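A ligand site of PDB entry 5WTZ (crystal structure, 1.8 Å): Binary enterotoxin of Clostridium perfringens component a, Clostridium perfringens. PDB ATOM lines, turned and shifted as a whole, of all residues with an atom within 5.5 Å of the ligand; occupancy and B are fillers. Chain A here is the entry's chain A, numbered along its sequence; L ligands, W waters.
The side-chain hydroxyl (OG1) of Thr 339 is in hydrogen-bond range of a nitrogen (N3) of the ligand (2.9 Å).
The side-chain amide nitrogen (ND2) of Asn 258 is in hydrogen-bond range of an oxygen (O1) of the ligand, at 3.0 Å.
O12 of the ligand lies within hydrogen-bond range of O of Leu 250 (2.8 Å).
The backbone NH of Gly 302 sits close to an oxygen (O6) of the ligand (3.3 Å).
OE2 of Glu 305 is in hydrogen-bond range of O6 of the ligand (2.7 Å).
NH2 of Arg 299 lies within salt-bridge range of O2 of the ligand.
An oxygen (O13) of the ligand lies within hydrogen-bond range of the side-chain carboxylate (OE1) of Glu 384.
The guanidinium group (NH2) of Arg 356 is in salt-bridge range of an oxygen (O9) of the ligand (2.9 Å).
The side-chain hydroxyl (OH) of Tyr 249 lies within hydrogen-bond range of the side-chain amide nitrogen (ND2) of Asn 258.
OG of Ser 342 is in hydrogen-bond range of OH of Tyr 249 (3.0 Å).
The guanidinium group (NH1) of Arg 299 is in hydrogen-bond range of the backbone carbonyl oxygen (O) of Ser 342 (2.9 Å).
The backbone NH (N) of Gly 302 is in hydrogen-bond range of the side-chain carboxylate (OE2) of Glu 305.
OD1 of Asn 258 is in hydrogen-bond range of N of Phe 340 (3.1 Å).
The backbone carbonyl oxygen (O) of Leu 262 lies within hydrogen-bond range of the side-chain amino group (NZ) of Lys 338.
The guanidinium group (NE) of Arg 299 is in salt-bridge range of the side-chain carboxylate (OE1) of Glu 305, at 3.0 Å.
The guanidinium group (NH1) of Arg 356 sits at hydrogen-bond distance from the backbone carbonyl oxygen (O) of Arg 300.
The backbone NH of Arg 300 sits close to a nitrogen (N7) of the ligand (2.9 Å).
CD1 of Tyr 254 touches O7 of the ligand, at 3.2 Å.
CD1 of Leu 262 touches N4 of the ligand, at 3.4 Å.
O of Asn 304 touches C9 of the ligand, 3.5 Å away.
Ser 342 touches the ligand (O to C19, 3.5 Å).
Thr 343 touches the ligand (O to C20, 3.4 Å).
Thr 344 touches the ligand (N to C19, 3.9 Å).
Ile 350 touches the ligand.
Phe 353 touches the ligand (CZ to O10, 3.4 Å).
Hydrophobic or aromatic side chains that line the ligand: Leu 250, Tyr 254, Leu 262, Ile 350 and Phe 353.
17 residues have an atom within 4 Å of the ligand: Leu 250, Tyr 254, Asn 258, Leu 262, Arg 299, Arg 300, Gly 302, Asn 304, Glu 305, Thr 339, Ser 342, Thr 343, Thr 344, Ile 350, Phe 353, Arg 356 and Glu 384.
The nearest printed residue that does not touch the ligand is Val 337 (4.2 Å).
Water W8 bridges N2 of the ligand (2.7 Å) and OG1 of Thr 339 (2.9 Å).
Water W11 bridges OD1 of Asn 304 (2.6 Å) and O5 of the ligand (2.8 Å).
Water W12 lies within hydrogen-bond range of O1 of the ligand, O of Thr 255 and O of Tyr 254.
Water W13 bridges the backbone NH (N) of Asn 304 (2.8 Å) and an oxygen (O6) of the ligand (2.9 Å).
Water W7 lies within hydrogen-bond range of a nitrogen (N3) of the ligand (3.0 Å) and the backbone NH (N) of Lys 338 (3.0 Å).
Water W3 lies within hydrogen-bond range of OD1 of Asn 304 (2.8 Å) and N5 of the ligand (3.1 Å).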
ATOM      1  N   TYR A 249     -22.805   0.795  33.262  1.00  0.00           N
ATOM      2  CA  TYR A 249     -22.441  -0.502  32.676  1.00  0.00           C
ATOM      3  C   TYR A 249     -23.517  -0.953  31.698  1.00  0.00           C
ATOM      4  O   TYR A 249     -23.228  -1.293  30.529  1.00  0.00           O
ATOM      5  CB  TYR A 249     -22.223  -1.555  33.764  1.00  0.00           C
ATOM      6  CG  TYR A 249     -22.005  -2.979  33.250  1.00  0.00           C
ATOM      7  CD1 TYR A 249     -23.091  -3.785  32.874  1.00  0.00           C
ATOM      8  CD2 TYR A 249     -20.730  -3.512  33.146  1.00  0.00           C
ATOM      9  CE1 TYR A 249     -22.900  -5.095  32.403  1.00  0.00           C
ATOM     10  CE2 TYR A 249     -20.535  -4.838  32.691  1.00  0.00           C
ATOM     11  CZ  TYR A 249     -21.629  -5.607  32.330  1.00  0.00           C
ATOM     12  OH  TYR A 249     -21.451  -6.897  31.858  1.00  0.00           O
ATOM     13  N   LEU A 250     -24.762  -0.941  32.165  1.00  0.00           N
ATOM     14  CA  LEU A 250     -25.850  -1.512  31.404  1.00  0.00           C
ATOM     15  C   LEU A 250     -26.130  -0.716  30.134  1.00  0.00           C
ATOM     16  O   LEU A 250     -26.518  -1.289  29.124  1.00  0.00           O
ATOM     17  CB  LEU A 250     -27.109  -1.603  32.269  1.00  0.00           C
ATOM     18  CG  LEU A 250     -27.076  -2.621  33.415  1.00  0.00           C
ATOM     19  CD1 LEU A 250     -28.305  -2.420  34.285  1.00  0.00           C
ATOM     20  CD2 LEU A 250     -26.975  -4.069  32.885  1.00  0.00           C
ATOM     21  N   GLY A 251     -25.906   0.584  30.189  1.00  0.00           N
ATOM     22  CA  GLY A 251     -26.192   1.460  29.066  1.00  0.00           C
ATOM     23  C   GLY A 251     -25.083   1.512  28.029  1.00  0.00           C
ATOM     24  O   GLY A 251     -25.177   2.281  27.075  1.00  0.00           O
ATOM     25  N   GLY A 252     -24.043   0.698  28.194  1.00  0.00           N
ATOM     26  CA  GLY A 252     -22.973   0.668  27.219  1.00  0.00           C
ATOM     27  C   GLY A 252     -21.555   0.751  27.789  1.00  0.00           C
ATOM     28  O   GLY A 252     -20.581   0.572  27.059  1.00  0.00           O
ATOM     29  N   TYR A 254     -20.307  -1.309  29.761  1.00  0.00           N
ATOM     30  CA  TYR A 254     -19.846  -2.721  29.809  1.00  0.00           C
ATOM     31  C   TYR A 254     -18.680  -2.978  28.853  1.00  0.00           C
ATOM     32  O   TYR A 254     -17.801  -3.788  29.145  1.00  0.00           O
ATOM     33  CB  TYR A 254     -21.003  -3.704  29.498  1.00  0.00           C
ATOM     34  CG  TYR A 254     -21.490  -3.621  28.068  1.00  0.00           C
ATOM     35  CD1 TYR A 254     -20.900  -4.382  27.067  1.00  0.00           C
ATOM     36  CD2 TYR A 254     -22.521  -2.753  27.731  1.00  0.00           C
ATOM     37  CE1 TYR A 254     -21.336  -4.282  25.747  1.00  0.00           C
ATOM     38  CE2 TYR A 254     -22.957  -2.643  26.414  1.00  0.00           C
ATOM     39  CZ  TYR A 254     -22.371  -3.411  25.434  1.00  0.00           C
ATOM     40  OH  TYR A 254     -22.824  -3.286  24.138  1.00  0.00           O
ATOM     41  N   THR A 255     -18.661  -2.280  27.722  1.00  0.00           N
ATOM     42  CA  THR A 255     -17.644  -2.521  26.686  1.00  0.00           C
ATOM     43  C   THR A 255     -16.249  -2.193  27.209  1.00  0.00           C
ATOM     44  O   THR A 255     -15.343  -3.020  27.116  1.00  0.00           O
ATOM     45  CB  THR A 255     -17.920  -1.690  25.437  1.00  0.00           C
ATOM     46  OG1 THR A 255     -19.148  -2.134  24.847  1.00  0.00           O
ATOM     47  CG2 THR A 255     -16.798  -1.855  24.425  1.00  0.00           C
ATOM     48  N   ASN A 258     -15.625  -4.451  30.777  1.00  0.00           N
ATOM     49  CA  ASN A 258     -15.288  -5.859  30.613  1.00  0.00           C
ATOM     50  C   ASN A 258     -13.976  -6.013  29.829  1.00  0.00           C
ATOM     51  O   ASN A 258     -13.197  -6.905  30.117  1.00  0.00           O
ATOM     52  CB  ASN A 258     -16.460  -6.636  29.978  1.00  0.00           C
ATOM     53  CG  ASN A 258     -17.578  -6.939  30.983  1.00  0.00           C
ATOM     54  OD1 ASN A 258     -17.343  -6.994  32.194  1.00  0.00           O
ATOM     55  ND2 ASN A 258     -18.788  -7.150  30.483  1.00  0.00           N
ATOM     56  N   LEU A 262     -10.789  -8.009  31.341  1.00  0.00           N
ATOM     57  CA  LEU A 262     -10.278  -9.168  30.611  1.00  0.00           C
ATOM     58  C   LEU A 262      -8.756  -9.108  30.442  1.00  0.00           C
ATOM     59  O   LEU A 262      -8.081 -10.114  30.660  1.00  0.00           O
ATOM     60  CB  LEU A 262     -10.970  -9.283  29.248  1.00  0.00           C
ATOM     61  CG  LEU A 262     -10.538 -10.481  28.410  1.00  0.00           C
ATOM     62  CD1 LEU A 262     -10.911 -11.824  29.066  1.00  0.00           C
ATOM     63  CD2 LEU A 262     -11.124 -10.375  27.007  1.00  0.00           C
ATOM     64  N   TYR A 298     -29.306 -17.386  30.944  1.00  0.00           N
ATOM     65  CA  TYR A 298     -28.818 -17.569  29.566  1.00  0.00           C
ATOM     66  C   TYR A 298     -27.883 -16.457  29.100  1.00  0.00           C
ATOM     67  O   TYR A 298     -27.931 -15.328  29.579  1.00  0.00           O
ATOM     68  CB  TYR A 298     -29.996 -17.663  28.590  1.00  0.00           C
ATOM     69  CG  TYR A 298     -30.983 -18.780  28.873  1.00  0.00           C
ATOM     70  CD1 TYR A 298     -32.060 -18.577  29.762  1.00  0.00           C
ATOM     71  CD2 TYR A 298     -30.845 -20.030  28.274  1.00  0.00           C
ATOM     72  CE1 TYR A 298     -32.966 -19.604  30.027  1.00  0.00           C
ATOM     73  CE2 TYR A 298     -31.741 -21.057  28.535  1.00  0.00           C
ATOM     74  CZ  TYR A 298     -32.780 -20.850  29.414  1.00  0.00           C
ATOM     75  OH  TYR A 298     -33.663 -21.870  29.651  1.00  0.00           O
ATOM     76  N   ARG A 299     -27.048 -16.751  28.104  1.00  0.00           N
ATOM     77  CA  ARG A 299     -26.180 -15.719  27.558  1.00  0.00           C
ATOM     78  C   ARG A 299     -25.880 -16.045  26.106  1.00  0.00           C
ATOM     79  O   ARG A 299     -25.526 -17.182  25.781  1.00  0.00           O
ATOM     80  CB  ARG A 299     -24.870 -15.609  28.346  1.00  0.00           C
ATOM     81  CG  ARG A 299     -23.923 -14.526  27.802  1.00  0.00           C
ATOM     82  CD  ARG A 299     -22.661 -14.343  28.660  1.00  0.00           C
ATOM     83  NE  ARG A 299     -21.663 -13.651  27.857  1.00  0.00           N
ATOM     84  CZ  ARG A 299     -21.713 -12.356  27.569  1.00  0.00           C
ATOM     85  NH1 ARG A 299     -22.689 -11.589  28.058  1.00  0.00           N
ATOM     86  NH2 ARG A 299     -20.771 -11.805  26.783  1.00  0.00           N
ATOM     87  N   ARG A 300     -26.060 -15.050  25.239  1.00  0.00           N
ATOM     88  CA  ARG A 300     -25.590 -15.129  23.866  1.00  0.00           C
ATOM     89  C   ARG A 300     -24.127 -14.717  23.881  1.00  0.00           C
ATOM     90  O   ARG A 300     -23.803 -13.543  24.106  1.00  0.00           O
ATOM     91  CB  ARG A 300     -26.452 -14.252  22.955  1.00  0.00           C
ATOM     92  CG  ARG A 300     -27.944 -14.618  23.029  1.00  0.00           C
ATOM     93  CD  ARG A 300     -28.159 -16.095  22.665  1.00  0.00           C
ATOM     94  NE  ARG A 300     -29.508 -16.611  22.910  1.00  0.00           N
ATOM     95  CZ  ARG A 300     -30.251 -17.230  21.995  1.00  0.00           C
ATOM     96  NH1 ARG A 300     -29.798 -17.374  20.760  1.00  0.00           N
ATOM     97  NH2 ARG A 300     -31.464 -17.690  22.292  1.00  0.00           N
ATOM     98  N   MET A 301     -23.238 -15.682  23.729  1.00  0.00           N
ATOM     99  CA  MET A 301     -21.813 -15.453  23.927  1.00  0.00           C
ATOM    100  C   MET A 301     -21.154 -15.205  22.577  1.00  0.00           C
ATOM    101  O   MET A 301     -21.536 -15.802  21.578  1.00  0.00           O
ATOM    102  CB  MET A 301     -21.144 -16.649  24.623  1.00  0.00           C
ATOM    103  CG  MET A 301     -21.896 -17.194  25.855  1.00  0.00           C
ATOM    104  SD  MET A 301     -21.202 -18.760  26.459  1.00  0.00           S
ATOM    105  CE  MET A 301     -19.804 -18.182  27.355  1.00  0.00           C
ATOM    106  N   GLY A 302     -20.159 -14.324  22.545  1.00  0.00           N
ATOM    107  CA  GLY A 302     -19.358 -14.155  21.344  1.00  0.00           C
ATOM    108  C   GLY A 302     -18.245 -15.206  21.292  1.00  0.00           C
ATOM    109  O   GLY A 302     -17.914 -15.813  22.321  1.00  0.00           O
ATOM    110  N   PRO A 303     -17.649 -15.398  20.107  1.00  0.00           N
ATOM    111  CA  PRO A 303     -16.619 -16.437  19.953  1.00  0.00           C
ATOM    112  C   PRO A 303     -15.383 -16.240  20.834  1.00  0.00           C
ATOM    113  O   PRO A 303     -14.797 -17.245  21.255  1.00  0.00           O
ATOM    114  CB  PRO A 303     -16.249 -16.322  18.465  1.00  0.00           C
ATOM    115  CG  PRO A 303     -16.608 -14.901  18.082  1.00  0.00           C
ATOM    116  CD  PRO A 303     -17.889 -14.678  18.845  1.00  0.00           C
ATOM    117  N   ASN A 304     -15.005 -14.992  21.120  1.00  0.00           N
ATOM    118  CA  ASN A 304     -13.839 -14.690  21.968  1.00  0.00           C
ATOM    119  C   ASN A 304     -13.899 -15.383  23.321  1.00  0.00           C
ATOM    120  O   ASN A 304     -12.868 -15.655  23.933  1.00  0.00           O
ATOM    121  CB  ASN A 304     -13.694 -13.194  22.240  1.00  0.00           C
ATOM    122  CG  ASN A 304     -13.316 -12.385  21.011  1.00  0.00           C
ATOM    123  OD1 ASN A 304     -13.177 -11.161  21.112  1.00  0.00           O
ATOM    124  ND2 ASN A 304     -13.164 -13.044  19.860  1.00  0.00           N
ATOM    125  N   GLU A 305     -15.105 -15.650  23.808  1.00  0.00           N
ATOM    126  CA  GLU A 305     -15.254 -16.259  25.128  1.00  0.00           C
ATOM    127  C   GLU A 305     -14.758 -17.703  25.143  1.00  0.00           C
ATOM    128  O   GLU A 305     -14.544 -18.277  26.208  1.00  0.00           O
ATOM    129  CB  GLU A 305     -16.703 -16.181  25.590  1.00  0.00           C
ATOM    130  CG  GLU A 305     -17.046 -14.734  25.965  1.00  0.00           C
ATOM    131  CD  GLU A 305     -18.527 -14.472  26.004  1.00  0.00           C
ATOM    132  OE1 GLU A 305     -19.193 -15.003  26.918  1.00  0.00           O
ATOM    133  OE2 GLU A 305     -19.034 -13.724  25.128  1.00  0.00           O
ATOM    134  N   VAL A 337     -13.674 -16.819  34.584  1.00  0.00           N
ATOM    135  CA  VAL A 337     -14.336 -15.707  33.925  1.00  0.00           C
ATOM    136  C   VAL A 337     -13.961 -14.389  34.627  1.00  0.00           C
ATOM    137  O   VAL A 337     -14.472 -14.071  35.705  1.00  0.00           O
ATOM    138  CB  VAL A 337     -15.868 -15.890  33.916  1.00  0.00           C
ATOM    139  CG1 VAL A 337     -16.546 -14.685  33.193  1.00  0.00           C
ATOM    140  CG2 VAL A 337     -16.250 -17.202  33.229  1.00  0.00           C
ATOM    141  N   LYS A 338     -13.071 -13.629  34.010  1.00  0.00           N
ATOM    142  CA  LYS A 338     -12.558 -12.408  34.617  1.00  0.00           C
ATOM    143  C   LYS A 338     -13.561 -11.254  34.570  1.00  0.00           C
ATOM    144  O   LYS A 338     -13.495 -10.316  35.357  1.00  0.00           O
ATOM    145  CB  LYS A 338     -11.242 -11.987  33.937  1.00  0.00           C
ATOM    146  CG  LYS A 338     -10.155 -13.065  33.972  1.00  0.00           C
ATOM    147  CD  LYS A 338      -8.879 -12.597  33.275  1.00  0.00           C
ATOM    148  CE  LYS A 338      -8.131 -11.593  34.135  1.00  0.00           C
ATOM    149  NZ  LYS A 338      -6.815 -11.204  33.554  1.00  0.00           N
ATOM    150  N   THR A 339     -14.497 -11.344  33.640  1.00  0.00           N
ATOM    151  CA  THR A 339     -15.437 -10.262  33.353  1.00  0.00           C
ATOM    152  C   THR A 339     -16.695 -10.343  34.220  1.00  0.00           C
ATOM    153  O   THR A 339     -16.963 -11.395  34.814  1.00  0.00           O
ATOM    154  CB  THR A 339     -15.867 -10.317  31.862  1.00  0.00           C
ATOM    155  OG1 THR A 339     -16.131 -11.681  31.505  1.00  0.00           O
ATOM    156  CG2 THR A 339     -14.766  -9.748  30.945  1.00  0.00           C
ATOM    157  N   PHE A 340     -17.444  -9.237  34.319  1.00  0.00           N
ATOM    158  CA  PHE A 340     -18.820  -9.324  34.773  1.00  0.00           C
ATOM    159  C   PHE A 340     -19.561 -10.107  33.707  1.00  0.00           C
ATOM    160  O   PHE A 340     -19.254  -9.989  32.512  1.00  0.00           O
ATOM    161  CB  PHE A 340     -19.491  -7.953  34.963  1.00  0.00           C
ATOM    162  CG  PHE A 340     -18.879  -7.089  36.039  1.00  0.00           C
ATOM    163  CD1 PHE A 340     -19.086  -7.382  37.389  1.00  0.00           C
ATOM    164  CD2 PHE A 340     -18.112  -5.997  35.707  1.00  0.00           C
ATOM    165  CE1 PHE A 340     -18.523  -6.596  38.380  1.00  0.00           C
ATOM    166  CE2 PHE A 340     -17.549  -5.192  36.704  1.00  0.00           C
ATOM    167  CZ  PHE A 340     -17.747  -5.503  38.045  1.00  0.00           C
ATOM    168  N   SER A 342     -23.045 -10.569  31.855  1.00  0.00           N
ATOM    169  CA  SER A 342     -24.396 -10.185  31.465  1.00  0.00           C
ATOM    170  C   SER A 342     -25.198 -11.409  30.979  1.00  0.00           C
ATOM    171  O   SER A 342     -24.890 -12.032  29.945  1.00  0.00           O
ATOM    172  CB  SER A 342     -24.373  -9.096  30.390  1.00  0.00           C
ATOM    173  OG  SER A 342     -24.168  -7.809  30.960  1.00  0.00           O
ATOM    174  N   THR A 343     -26.214 -11.764  31.741  1.00  0.00           N
ATOM    175  CA  THR A 343     -27.066 -12.906  31.395  1.00  0.00           C
ATOM    176  C   THR A 343     -28.519 -12.473  31.358  1.00  0.00           C
ATOM    177  O   THR A 343     -28.885 -11.455  31.933  1.00  0.00           O
ATOM    178  CB  THR A 343     -26.953 -14.092  32.408  1.00  0.00           C
ATOM    179  OG1 THR A 343     -27.737 -13.821  33.578  1.00  0.00           O
ATOM    180  CG2 THR A 343     -25.508 -14.379  32.788  1.00  0.00           C
ATOM    181  N   THR A 344     -29.337 -13.241  30.649  1.00  0.00           N
ATOM    182  CA  THR A 344     -30.771 -12.991  30.592  1.00  0.00           C
ATOM    183  C   THR A 344     -31.493 -14.263  31.029  1.00  0.00           C
ATOM    184  O   THR A 344     -31.164 -15.365  30.592  1.00  0.00           O
ATOM    185  CB  THR A 344     -31.220 -12.546  29.177  1.00  0.00           C
ATOM    186  OG1 THR A 344     -32.640 -12.407  29.137  1.00  0.00           O
ATOM    187  CG2 THR A 344     -30.810 -13.564  28.096  1.00  0.00           C
ATOM    188  N   ILE A 350     -31.795 -12.532  21.413  1.00  0.00           N
ATOM    189  CA  ILE A 350     -31.769 -11.076  21.546  1.00  0.00           C
ATOM    190  C   ILE A 350     -31.351 -10.458  20.222  1.00  0.00           C
ATOM    191  O   ILE A 350     -30.345 -10.884  19.645  1.00  0.00           O
ATOM    192  CB  ILE A 350     -30.808 -10.627  22.668  1.00  0.00           C
ATOM    193  CG1 ILE A 350     -31.264 -11.172  24.026  1.00  0.00           C
ATOM    194  CG2 ILE A 350     -30.703  -9.108  22.697  1.00  0.00           C
ATOM    195  CD1 ILE A 350     -30.191 -11.079  25.111  1.00  0.00           C
ATOM    196  N   PHE A 353     -27.809  -9.522  19.374  1.00  0.00           N
ATOM    197  CA  PHE A 353     -26.872 -10.644  19.420  1.00  0.00           C
ATOM    198  C   PHE A 353     -27.423 -11.875  18.713  1.00  0.00           C
ATOM    199  O   PHE A 353     -27.091 -13.000  19.087  1.00  0.00           O
ATOM    200  CB  PHE A 353     -26.526 -10.973  20.871  1.00  0.00           C
ATOM    201  CG  PHE A 353     -26.198  -9.760  21.708  1.00  0.00           C
ATOM    202  CD1 PHE A 353     -25.131  -8.948  21.359  1.00  0.00           C
ATOM    203  CD2 PHE A 353     -26.975  -9.416  22.811  1.00  0.00           C
ATOM    204  CE1 PHE A 353     -24.824  -7.810  22.102  1.00  0.00           C
ATOM    205  CE2 PHE A 353     -26.676  -8.278  23.557  1.00  0.00           C
ATOM    206  CZ  PHE A 353     -25.601  -7.475  23.202  1.00  0.00           C
ATOM    207  N   ARG A 356     -24.942 -14.620  17.202  1.00  0.00           N
ATOM    208  CA  ARG A 356     -23.994 -15.345  18.057  1.00  0.00           C
ATOM    209  C   ARG A 356     -24.393 -16.833  18.140  1.00  0.00           C
ATOM    210  O   ARG A 356     -25.570 -17.151  18.350  1.00  0.00           O
ATOM    211  CB  ARG A 356     -23.918 -14.732  19.450  1.00  0.00           C
ATOM    212  CG  ARG A 356     -23.389 -13.289  19.444  1.00  0.00           C
ATOM    213  CD  ARG A 356     -23.033 -12.812  20.828  1.00  0.00           C
ATOM    214  NE  ARG A 356     -22.528 -11.451  20.750  1.00  0.00           N
ATOM    215  CZ  ARG A 356     -22.305 -10.657  21.793  1.00  0.00           C
ATOM    216  NH1 ARG A 356     -22.568 -11.069  23.024  1.00  0.00           N
ATOM    217  NH2 ARG A 356     -21.844  -9.427  21.599  1.00  0.00           N
ATOM    218  N   GLU A 382     -36.297  -5.826  29.429  1.00  0.00           N
ATOM    219  CA  GLU A 382     -35.025  -6.436  29.805  1.00  0.00           C
ATOM    220  C   GLU A 382     -35.245  -7.363  31.004  1.00  0.00           C
ATOM    221  O   GLU A 382     -36.146  -7.139  31.823  1.00  0.00           O
ATOM    222  CB  GLU A 382     -33.997  -5.362  30.130  1.00  0.00           C
ATOM    223  CG  GLU A 382     -33.812  -4.327  29.021  1.00  0.00           C
ATOM    224  CD  GLU A 382     -32.479  -4.444  28.319  1.00  0.00           C
ATOM    225  OE1 GLU A 382     -32.056  -3.459  27.667  1.00  0.00           O
ATOM    226  OE2 GLU A 382     -31.849  -5.522  28.398  1.00  0.00           O
ATOM    227  N   GLU A 384     -32.362  -9.070  32.809  1.00  0.00           N
ATOM    228  CA  GLU A 384     -30.959  -9.372  33.001  1.00  0.00           C
ATOM    229  C   GLU A 384     -30.601  -9.741  34.446  1.00  0.00           C
ATOM    230  O   GLU A 384     -31.017  -9.055  35.414  1.00  0.00           O
ATOM    231  CB  GLU A 384     -30.083  -8.196  32.563  1.00  0.00           C
ATOM    232  CG  GLU A 384     -28.608  -8.431  32.808  1.00  0.00           C
ATOM    233  CD  GLU A 384     -27.694  -7.466  32.041  1.00  0.00           C
ATOM    234  OE1 GLU A 384     -28.198  -6.580  31.327  1.00  0.00           O
ATOM    235  OE2 GLU A 384     -26.463  -7.624  32.145  1.00  0.00           O
HETATM  236  P1  LIG L   1     -19.800  -8.202  26.925  1.00  0.00           P
HETATM  237  O1  LIG L   1     -18.958  -7.085  27.485  1.00  0.00           O
HETATM  238  O2  LIG L   1     -20.062  -9.439  27.744  1.00  0.00           O
HETATM  239  O3  LIG L   1     -19.175  -8.716  25.532  1.00  0.00           O
HETATM  240  C1  LIG L   1     -18.580  -7.836  24.574  1.00  0.00           C
HETATM  241  C2  LIG L   1     -17.578  -8.610  23.736  1.00  0.00           C
HETATM  242  O4  LIG L   1     -16.543  -9.067  24.605  1.00  0.00           O
HETATM  243  C3  LIG L   1     -18.210  -9.834  23.077  1.00  0.00           C
HETATM  244  O5  LIG L   1     -17.629  -9.999  21.775  1.00  0.00           O
HETATM  245  C4  LIG L   1     -17.793 -10.974  24.000  1.00  0.00           C
HETATM  246  O6  LIG L   1     -17.668 -12.228  23.316  1.00  0.00           O
HETATM  247  C5  LIG L   1     -16.453 -10.498  24.554  1.00  0.00           C
HETATM  248  N1  LIG L   1     -16.279 -11.032  25.929  1.00  0.00           N
HETATM  249  C6  LIG L   1     -17.102 -10.857  26.971  1.00  0.00           C
HETATM  250  N2  LIG L   1     -16.622 -11.508  28.071  1.00  0.00           N
HETATM  251  C7  LIG L   1     -15.498 -12.126  27.704  1.00  0.00           C
HETATM  252  C8  LIG L   1     -14.493 -12.987  28.357  1.00  0.00           C
HETATM  253  N3  LIG L   1     -14.627 -13.328  29.657  1.00  0.00           N
HETATM  254  N4  LIG L   1     -13.459 -13.444  27.609  1.00  0.00           N
HETATM  255  C9  LIG L   1     -13.313 -13.105  26.315  1.00  0.00           C
HETATM  256  N5  LIG L   1     -14.190 -12.315  25.654  1.00  0.00           N
HETATM  257  C10 LIG L   1     -15.279 -11.823  26.288  1.00  0.00           C
HETATM  258  O7  LIG L   1     -21.204  -7.556  26.536  1.00  0.00           O
HETATM  259  P2  LIG L   1     -22.372  -8.144  25.598  1.00  0.00           P
HETATM  260  O8  LIG L   1     -22.956  -9.368  26.280  1.00  0.00           O
HETATM  261  O9  LIG L   1     -21.862  -8.211  24.184  1.00  0.00           O
HETATM  262  O10 LIG L   1     -23.407  -6.915  25.682  1.00  0.00           O
HETATM  263  C11 LIG L   1     -23.863  -6.401  26.936  1.00  0.00           C
HETATM  264  C12 LIG L   1     -25.077  -5.519  26.693  1.00  0.00           C
HETATM  265  O11 LIG L   1     -26.202  -6.337  26.391  1.00  0.00           O
HETATM  266  C13 LIG L   1     -25.450  -4.782  27.969  1.00  0.00           C
HETATM  267  O12 LIG L   1     -26.203  -3.622  27.594  1.00  0.00           O
HETATM  268  C14 LIG L   1     -26.347  -5.771  28.680  1.00  0.00           C
HETATM  269  O13 LIG L   1     -27.279  -5.112  29.547  1.00  0.00           O
HETATM  270  C15 LIG L   1     -27.031  -6.518  27.531  1.00  0.00           C
HETATM  271  N6  LIG L   1     -27.210  -7.965  27.777  1.00  0.00           N
HETATM  272  C16 LIG L   1     -26.595  -8.881  27.004  1.00  0.00           C
HETATM  273  C17 LIG L   1     -26.770 -10.246  27.252  1.00  0.00           C
HETATM  274  C18 LIG L   1     -26.114 -11.296  26.402  1.00  0.00           C
HETATM  275  O14 LIG L   1     -25.054 -11.073  25.794  1.00  0.00           O
HETATM  276  N7  LIG L   1     -26.746 -12.456  26.310  1.00  0.00           N
HETATM  277  C19 LIG L   1     -27.600 -10.684  28.279  1.00  0.00           C
HETATM  278  C20 LIG L   1     -28.217  -9.717  29.058  1.00  0.00           C
HETATM  279  C21 LIG L   1     -28.007  -8.366  28.784  1.00  0.00           C
HETATM  280  O   HOH W   1     -26.899  -2.872  25.105  1.00  0.00           O
HETATM  281  O   HOH W   2     -13.604 -16.533  30.367  1.00  0.00           O
HETATM  282  O   HOH W   3     -12.572 -10.453  23.803  1.00  0.00           O
HETATM  283  O   HOH W   4     -16.143  -5.523  24.042  1.00  0.00           O
HETATM  284  O   HOH W   5     -11.441 -15.176  27.871  1.00  0.00           O
HETATM  285  O   HOH W   6     -15.988 -16.392  29.139  1.00  0.00           O
HETATM  286  O   HOH W   7     -12.283 -14.273  31.214  1.00  0.00           O
HETATM  287  O   HOH W   8     -18.483 -12.337  29.907  1.00  0.00           O
HETATM  288  O   HOH W   9     -29.264  -3.274  28.881  1.00  0.00           O
HETATM  289  O   HOH W  10     -29.996  -7.173  25.982  1.00  0.00           O
HETATM  290  O   HOH W  11     -14.964  -9.271  21.450  1.00  0.00           O
HETATM  291  O   HOH W  12     -16.505  -5.857  26.706  1.00  0.00           O
HETATM  292  O   HOH W  13     -16.422 -12.550  20.752  1.00  0.00           O
HETATM  293  O   HOH W  14     -30.490  -5.375  30.613  1.00  0.00           O
HETATM  294  O   HOH W  15     -20.465 -10.311  30.185  1.00  0.00           O
